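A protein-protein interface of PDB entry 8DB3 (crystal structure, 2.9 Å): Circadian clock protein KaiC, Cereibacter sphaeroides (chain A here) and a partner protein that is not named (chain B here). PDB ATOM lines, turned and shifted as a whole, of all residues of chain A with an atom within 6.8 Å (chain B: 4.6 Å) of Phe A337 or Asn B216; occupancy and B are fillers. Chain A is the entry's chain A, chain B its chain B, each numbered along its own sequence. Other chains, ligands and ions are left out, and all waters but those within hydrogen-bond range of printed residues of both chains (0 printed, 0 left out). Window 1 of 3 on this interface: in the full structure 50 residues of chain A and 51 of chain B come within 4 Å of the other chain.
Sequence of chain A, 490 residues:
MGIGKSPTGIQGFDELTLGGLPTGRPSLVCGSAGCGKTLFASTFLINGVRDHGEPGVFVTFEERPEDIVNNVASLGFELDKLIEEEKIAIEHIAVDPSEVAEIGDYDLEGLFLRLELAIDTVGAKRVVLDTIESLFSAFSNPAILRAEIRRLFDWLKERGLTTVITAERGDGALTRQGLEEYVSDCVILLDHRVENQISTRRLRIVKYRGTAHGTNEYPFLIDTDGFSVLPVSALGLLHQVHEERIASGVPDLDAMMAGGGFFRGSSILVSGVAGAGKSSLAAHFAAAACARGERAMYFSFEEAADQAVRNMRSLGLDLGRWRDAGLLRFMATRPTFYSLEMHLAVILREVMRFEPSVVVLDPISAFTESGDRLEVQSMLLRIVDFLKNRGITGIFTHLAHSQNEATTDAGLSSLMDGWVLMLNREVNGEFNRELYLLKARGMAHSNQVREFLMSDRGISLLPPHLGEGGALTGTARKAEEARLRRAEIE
Among the printed residues, merely in contact across the chains: His A192 with Arg B204, His A192 with Thr B215, Val A194 with Arg B204, Val A194 with Glu B217, Gln A197 with Asn B216, Ile A198 with Asn B216 and Ser A199 with Arg B204.
The backbone NH (N) of Ser A199 lies within hydrogen-bond range of the side-chain amide oxygen (OD1) of Asn B216 (3.0 Å). The backbone NH (N) of Glu B217 lies within hydrogen-bond range of the backbone carbonyl oxygen (O) of Gln A197 (3.0 Å). The backbone carbonyl oxygen (O) of Phe A337 sits at hydrogen-bond distance from the side-chain amide nitrogen (ND2) of Asn B216 (3.0 Å). The side-chain hydroxyl of Ser A199 lies within hydrogen-bond range of the backbone carbonyl oxygen of Thr B215 (2.6 Å).
Phe A337 touches just one residue of chain B: Asn B216 (3.0 Å). Of chain A, only Gln A197 (3.2 Å), Ile A198 (3.7 Å), Ser A199 (3.0 Å) and Phe A337 (3.0 Å) come within 4 Å of Asn B216. Printed residues of chain B within 4 Å of Ser A199: Arg B204, Thr B215 and Asn B216. Of the printed residues of chain A, Arg B204 touches His A192 (3.1 Å), Val A194 (3.8 Å) and Ser A199 (3.9 Å). Printed residues of chain A within 4 Å of Thr B215: His A192 (3.4 Å) and Ser A199 (2.6 Å). Tyr B218 touches none of the printed residues of chain A. Ser A339 touches none of the printed residues of chain B. The nearest residue of chain B that does not touch Phe A337 is Tyr B218 (4.5 Å). The nearest printed residue of chain B that does not touch Ile A198 is Glu B217 (5.0 Å).
Of the 7 printed residues of chain B, 4 touch a printed residue of chain A. Of the 13 printed residues of chain A, 6 touch a printed residue of chain B. Hydrophobic or aromatic side chains of chain A within 4 Å of the printed part of chain B: His A192 and Val A194. Along chain A the printed residues that touch a printed residue of chain B span positions 192 to 337. Among the printed residues, no Asp or Glu carboxylate lies within 4 Å of a Lys or Arg side-chain nitrogen of the other chain.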
ATOM      1  N   HIS A 192      -4.273 -21.539   5.478  1.00  0.00           N
ATOM      2  CA  HIS A 192      -4.205 -21.059   6.855  1.00  0.00           C
ATOM      3  C   HIS A 192      -3.491 -19.711   6.830  1.00  0.00           C
ATOM      4  O   HIS A 192      -2.260 -19.647   6.864  1.00  0.00           O
ATOM      5  CB  HIS A 192      -3.487 -22.072   7.735  1.00  0.00           C
ATOM      6  CG  HIS A 192      -3.848 -21.966   9.181  1.00  0.00           C
ATOM      7  ND1 HIS A 192      -4.565 -22.937   9.848  1.00  0.00           N
ATOM      8  CD2 HIS A 192      -3.597 -20.995  10.087  1.00  0.00           C
ATOM      9  CE1 HIS A 192      -4.731 -22.568  11.106  1.00  0.00           C
ATOM     10  NE2 HIS A 192      -4.158 -21.391  11.274  1.00  0.00           N
ATOM     11  N   VAL A 194      -2.592 -15.755   7.931  1.00  0.00           N
ATOM     12  CA  VAL A 194      -2.329 -14.987   9.142  1.00  0.00           C
ATOM     13  C   VAL A 194      -2.583 -13.510   8.876  1.00  0.00           C
ATOM     14  O   VAL A 194      -2.173 -12.969   7.841  1.00  0.00           O
ATOM     15  CB  VAL A 194      -0.887 -15.211   9.638  1.00  0.00           C
ATOM     16  CG1 VAL A 194      -0.432 -14.058  10.522  1.00  0.00           C
ATOM     17  CG2 VAL A 194      -0.780 -16.528  10.384  1.00  0.00           C
ATOM     18  N   GLN A 197      -1.340 -11.457  13.469  1.00  0.00           N
ATOM     19  CA  GLN A 197      -0.937 -12.577  14.312  1.00  0.00           C
ATOM     20  C   GLN A 197      -2.068 -13.562  14.576  1.00  0.00           C
ATOM     21  O   GLN A 197      -1.890 -14.495  15.371  1.00  0.00           O
ATOM     22  CB  GLN A 197      -0.372 -12.094  15.655  1.00  0.00           C
ATOM     23  CG  GLN A 197       1.006 -11.447  15.576  1.00  0.00           C
ATOM     24  CD  GLN A 197       1.476 -10.899  16.916  1.00  0.00           C
ATOM     25  OE1 GLN A 197       2.563 -11.229  17.394  1.00  0.00           O
ATOM     26  NE2 GLN A 197       0.651 -10.058  17.532  1.00  0.00           N
ATOM     27  N   ILE A 198      -3.225 -13.390  13.938  1.00  0.00           N
ATOM     28  CA  ILE A 198      -4.368 -14.277  14.113  1.00  0.00           C
ATOM     29  C   ILE A 198      -4.540 -15.084  12.834  1.00  0.00           C
ATOM     30  O   ILE A 198      -4.635 -14.514  11.739  1.00  0.00           O
ATOM     31  CB  ILE A 198      -5.652 -13.500  14.444  1.00  0.00           C
ATOM     32  CG1 ILE A 198      -5.415 -12.540  15.607  1.00  0.00           C
ATOM     33  CG2 ILE A 198      -6.774 -14.463  14.797  1.00  0.00           C
ATOM     34  CD1 ILE A 198      -6.517 -11.512  15.779  1.00  0.00           C
ATOM     35  N   SER A 199      -4.590 -16.403  12.971  1.00  0.00           N
ATOM     36  CA  SER A 199      -4.578 -17.313  11.833  1.00  0.00           C
ATOM     37  C   SER A 199      -5.975 -17.872  11.607  1.00  0.00           C
ATOM     38  O   SER A 199      -6.566 -18.465  12.516  1.00  0.00           O
ATOM     39  CB  SER A 199      -3.573 -18.445  12.061  1.00  0.00           C
ATOM     40  OG  SER A 199      -2.383 -17.958  12.665  1.00  0.00           O
ATOM     41  N   THR A 200      -6.489 -17.696  10.392  1.00  0.00           N
ATOM     42  CA  THR A 200      -7.816 -18.154  10.002  1.00  0.00           C
ATOM     43  C   THR A 200      -7.677 -19.208   8.913  1.00  0.00           C
ATOM     44  O   THR A 200      -6.907 -19.026   7.964  1.00  0.00           O
ATOM     45  CB  THR A 200      -8.669 -16.982   9.504  1.00  0.00           C
ATOM     46  OG1 THR A 200      -8.728 -15.970  10.520  1.00  0.00           O
ATOM     47  CG2 THR A 200     -10.078 -17.436   9.163  1.00  0.00           C
ATOM     48  N   ARG A 334     -13.089 -13.030  24.632  1.00  0.00           N
ATOM     49  CA  ARG A 334     -12.282 -11.876  24.266  1.00  0.00           C
ATOM     50  C   ARG A 334     -12.226 -11.760  22.749  1.00  0.00           C
ATOM     51  O   ARG A 334     -11.838 -12.724  22.072  1.00  0.00           O
ATOM     52  CB  ARG A 334     -10.860 -11.998  24.843  1.00  0.00           C
ATOM     53  CG  ARG A 334     -10.691 -11.356  26.222  1.00  0.00           C
ATOM     54  CD  ARG A 334     -10.914  -9.846  26.174  1.00  0.00           C
ATOM     55  NE  ARG A 334     -10.675  -9.210  27.468  1.00  0.00           N
ATOM     56  CZ  ARG A 334     -11.254  -8.088  27.873  1.00  0.00           C
ATOM     57  NH1 ARG A 334     -12.109  -7.434  27.105  1.00  0.00           N
ATOM     58  NH2 ARG A 334     -10.973  -7.614  29.084  1.00  0.00           N
ATOM     59  N   PRO A 335     -12.590 -10.607  22.175  1.00  0.00           N
ATOM     60  CA  PRO A 335     -12.741 -10.545  20.713  1.00  0.00           C
ATOM     61  C   PRO A 335     -11.466 -10.824  19.934  1.00  0.00           C
ATOM     62  O   PRO A 335     -11.540 -11.339  18.811  1.00  0.00           O
ATOM     63  CB  PRO A 335     -13.230  -9.106  20.466  1.00  0.00           C
ATOM     64  CG  PRO A 335     -13.746  -8.624  21.784  1.00  0.00           C
ATOM     65  CD  PRO A 335     -12.922  -9.326  22.826  1.00  0.00           C
ATOM     66  N   THR A 336     -10.298 -10.504  20.491  1.00  0.00           N
ATOM     67  CA  THR A 336      -9.055 -10.464  19.733  1.00  0.00           C
ATOM     68  C   THR A 336      -8.319 -11.798  19.710  1.00  0.00           C
ATOM     69  O   THR A 336      -7.092 -11.818  19.531  1.00  0.00           O
ATOM     70  CB  THR A 336      -8.138  -9.378  20.303  1.00  0.00           C
ATOM     71  OG1 THR A 336      -7.797  -9.703  21.658  1.00  0.00           O
ATOM     72  CG2 THR A 336      -8.825  -8.021  20.270  1.00  0.00           C
ATOM     73  N   PHE A 337      -9.027 -12.917  19.862  1.00  0.00           N
ATOM     74  CA  PHE A 337      -8.379 -14.215  20.019  1.00  0.00           C
ATOM     75  C   PHE A 337      -8.407 -15.050  18.743  1.00  0.00           C
ATOM     76  O   PHE A 337      -7.351 -15.342  18.171  1.00  0.00           O
ATOM     77  CB  PHE A 337      -9.039 -14.990  21.172  1.00  0.00           C
ATOM     78  CG  PHE A 337      -8.519 -16.392  21.344  1.00  0.00           C
ATOM     79  CD1 PHE A 337      -7.159 -16.656  21.271  1.00  0.00           C
ATOM     80  CD2 PHE A 337      -9.388 -17.445  21.579  1.00  0.00           C
ATOM     81  CE1 PHE A 337      -6.678 -17.944  21.428  1.00  0.00           C
ATOM     82  CE2 PHE A 337      -8.913 -18.735  21.737  1.00  0.00           C
ATOM     83  CZ  PHE A 337      -7.555 -18.984  21.661  1.00  0.00           C
ATOM     84  N   TYR A 338      -9.596 -15.444  18.286  1.00  0.00           N
ATOM     85  CA  TYR A 338      -9.716 -16.478  17.269  1.00  0.00           C
ATOM     86  C   TYR A 338     -10.428 -16.027  16.003  1.00  0.00           C
ATOM     87  O   TYR A 338     -10.806 -16.879  15.203  1.00  0.00           O
ATOM     88  CB  TYR A 338     -10.443 -17.699  17.852  1.00  0.00           C
ATOM     89  N   SER A 339     -10.614 -14.721  15.806  1.00  0.00           N
ATOM     90  CA  SER A 339     -11.210 -14.129  14.612  1.00  0.00           C
ATOM     91  C   SER A 339     -12.738 -14.136  14.643  1.00  0.00           C
ATOM     92  O   SER A 339     -13.368 -14.902  15.388  1.00  0.00           O
ATOM     93  CB  SER A 339     -10.739 -14.831  13.332  1.00  0.00           C
ATOM     94  OG  SER A 339     -11.623 -14.549  12.245  1.00  0.00           O
ATOM     95  N   HIS A 343     -15.567 -16.684  16.315  1.00  0.00           N
ATOM     96  CA  HIS A 343     -16.484 -16.222  17.351  1.00  0.00           C
ATOM     97  C   HIS A 343     -17.905 -16.607  16.956  1.00  0.00           C
ATOM     98  O   HIS A 343     -18.530 -17.459  17.602  1.00  0.00           O
ATOM     99  CB  HIS A 343     -16.365 -14.719  17.555  1.00  0.00           C
ATOM    100  CG  HIS A 343     -15.336 -14.333  18.570  1.00  0.00           C
ATOM    101  ND1 HIS A 343     -13.993 -14.589  18.398  1.00  0.00           N
ATOM    102  CD2 HIS A 343     -15.452 -13.721  19.772  1.00  0.00           C
ATOM    103  CE1 HIS A 343     -13.325 -14.146  19.448  1.00  0.00           C
ATOM    104  NE2 HIS A 343     -14.187 -13.615  20.296  1.00  0.00           N
ATOM    105  N   LEU B 203       7.012 -17.041  17.014  1.00  0.00           N
ATOM    106  CA  LEU B 203       6.930 -18.476  16.790  1.00  0.00           C
ATOM    107  C   LEU B 203       5.549 -18.796  16.240  1.00  0.00           C
ATOM    108  O   LEU B 203       4.551 -18.197  16.655  1.00  0.00           O
ATOM    109  CB  LEU B 203       7.176 -19.238  18.089  1.00  0.00           C
ATOM    110  CG  LEU B 203       6.827 -20.724  18.133  1.00  0.00           C
ATOM    111  CD1 LEU B 203       7.861 -21.462  18.978  1.00  0.00           C
ATOM    112  CD2 LEU B 203       5.428 -20.954  18.676  1.00  0.00           C
ATOM    113  N   ARG B 204       5.494 -19.728  15.296  1.00  0.00           N
ATOM    114  CA  ARG B 204       4.218 -20.179  14.764  1.00  0.00           C
ATOM    115  C   ARG B 204       4.255 -21.683  14.563  1.00  0.00           C
ATOM    116  O   ARG B 204       5.250 -22.226  14.083  1.00  0.00           O
ATOM    117  CB  ARG B 204       3.882 -19.490  13.438  1.00  0.00           C
ATOM    118  CG  ARG B 204       2.396 -19.262  13.239  1.00  0.00           C
ATOM    119  CD  ARG B 204       2.071 -19.013  11.782  1.00  0.00           C
ATOM    120  NE  ARG B 204       0.881 -19.749  11.369  1.00  0.00           N
ATOM    121  CZ  ARG B 204       0.618 -20.104  10.120  1.00  0.00           C
ATOM    122  NH1 ARG B 204       1.444 -19.811   9.130  1.00  0.00           N
ATOM    123  NH2 ARG B 204      -0.503 -20.768   9.857  1.00  0.00           N
ATOM    124  N   GLY B 214      -1.894 -24.136  19.301  1.00  0.00           N
ATOM    125  CA  GLY B 214      -2.020 -22.728  18.991  1.00  0.00           C
ATOM    126  C   GLY B 214      -1.632 -22.398  17.567  1.00  0.00           C
ATOM    127  O   GLY B 214      -0.455 -22.459  17.202  1.00  0.00           O
ATOM    128  N   THR B 215      -2.625 -22.041  16.752  1.00  0.00           N
ATOM    129  CA  THR B 215      -2.392 -21.740  15.349  1.00  0.00           C
ATOM    130  C   THR B 215      -1.925 -20.311  15.112  1.00  0.00           C
ATOM    131  O   THR B 215      -1.454 -20.007  14.011  1.00  0.00           O
ATOM    132  CB  THR B 215      -3.676 -21.987  14.548  1.00  0.00           C
ATOM    133  OG1 THR B 215      -4.799 -21.487  15.284  1.00  0.00           O
ATOM    134  CG2 THR B 215      -3.862 -23.474  14.281  1.00  0.00           C
ATOM    135  N   ASN B 216      -2.038 -19.436  16.107  1.00  0.00           N
ATOM    136  CA  ASN B 216      -1.699 -18.036  15.929  1.00  0.00           C
ATOM    137  C   ASN B 216      -0.188 -17.825  16.032  1.00  0.00           C
ATOM    138  O   ASN B 216       0.571 -18.718  16.421  1.00  0.00           O
ATOM    139  CB  ASN B 216      -2.418 -17.177  16.969  1.00  0.00           C
ATOM    140  CG  ASN B 216      -3.914 -17.102  16.730  1.00  0.00           C
ATOM    141  OD1 ASN B 216      -4.417 -17.567  15.708  1.00  0.00           O
ATOM    142  ND2 ASN B 216      -4.633 -16.512  17.679  1.00  0.00           N
ATOM    143  N   GLU B 217       0.242 -16.621  15.661  1.00  0.00           N
ATOM    144  CA  GLU B 217       1.621 -16.201  15.863  1.00  0.00           C
ATOM    145  C   GLU B 217       1.806 -15.747  17.305  1.00  0.00           C
ATOM    146  O   GLU B 217       0.975 -15.014  17.849  1.00  0.00           O
ATOM    147  CB  GLU B 217       1.983 -15.066  14.908  1.00  0.00           C
ATOM    148  CG  GLU B 217       2.337 -15.514  13.503  1.00  0.00           C
ATOM    149  CD  GLU B 217       2.935 -14.393  12.677  1.00  0.00           C
ATOM    150  OE1 GLU B 217       2.543 -13.225  12.886  1.00  0.00           O
ATOM    151  OE2 GLU B 217       3.801 -14.682  11.825  1.00  0.00           O
ATOM    152  N   TYR B 218       2.901 -16.176  17.926  1.00  0.00           N
ATOM    153  CA  TYR B 218       3.131 -15.929  19.347  1.00  0.00           C
ATOM    154  C   TYR B 218       4.517 -15.340  19.540  1.00  0.00           C
ATOM    155  O   TYR B 218       5.520 -15.994  19.197  1.00  0.00           O
ATOM    156  CB  TYR B 218       2.956 -17.234  20.130  1.00  0.00           C
ATOM    157  CG  TYR B 218       1.520 -17.709  20.162  1.00  0.00           C
ATOM    158  CD1 TYR B 218       0.520 -16.907  20.700  1.00  0.00           C
ATOM    159  CD2 TYR B 218       1.156 -18.946  19.643  1.00  0.00           C
ATOM    160  CE1 TYR B 218      -0.800 -17.328  20.731  1.00  0.00           C
ATOM    161  CE2 TYR B 218      -0.161 -19.377  19.673  1.00  0.00           C
ATOM    162  CZ  TYR B 218      -1.137 -18.564  20.216  1.00  0.00           C
ATOM    163  OH  TYR B 218      -2.451 -18.981  20.247  1.00  0.00           O
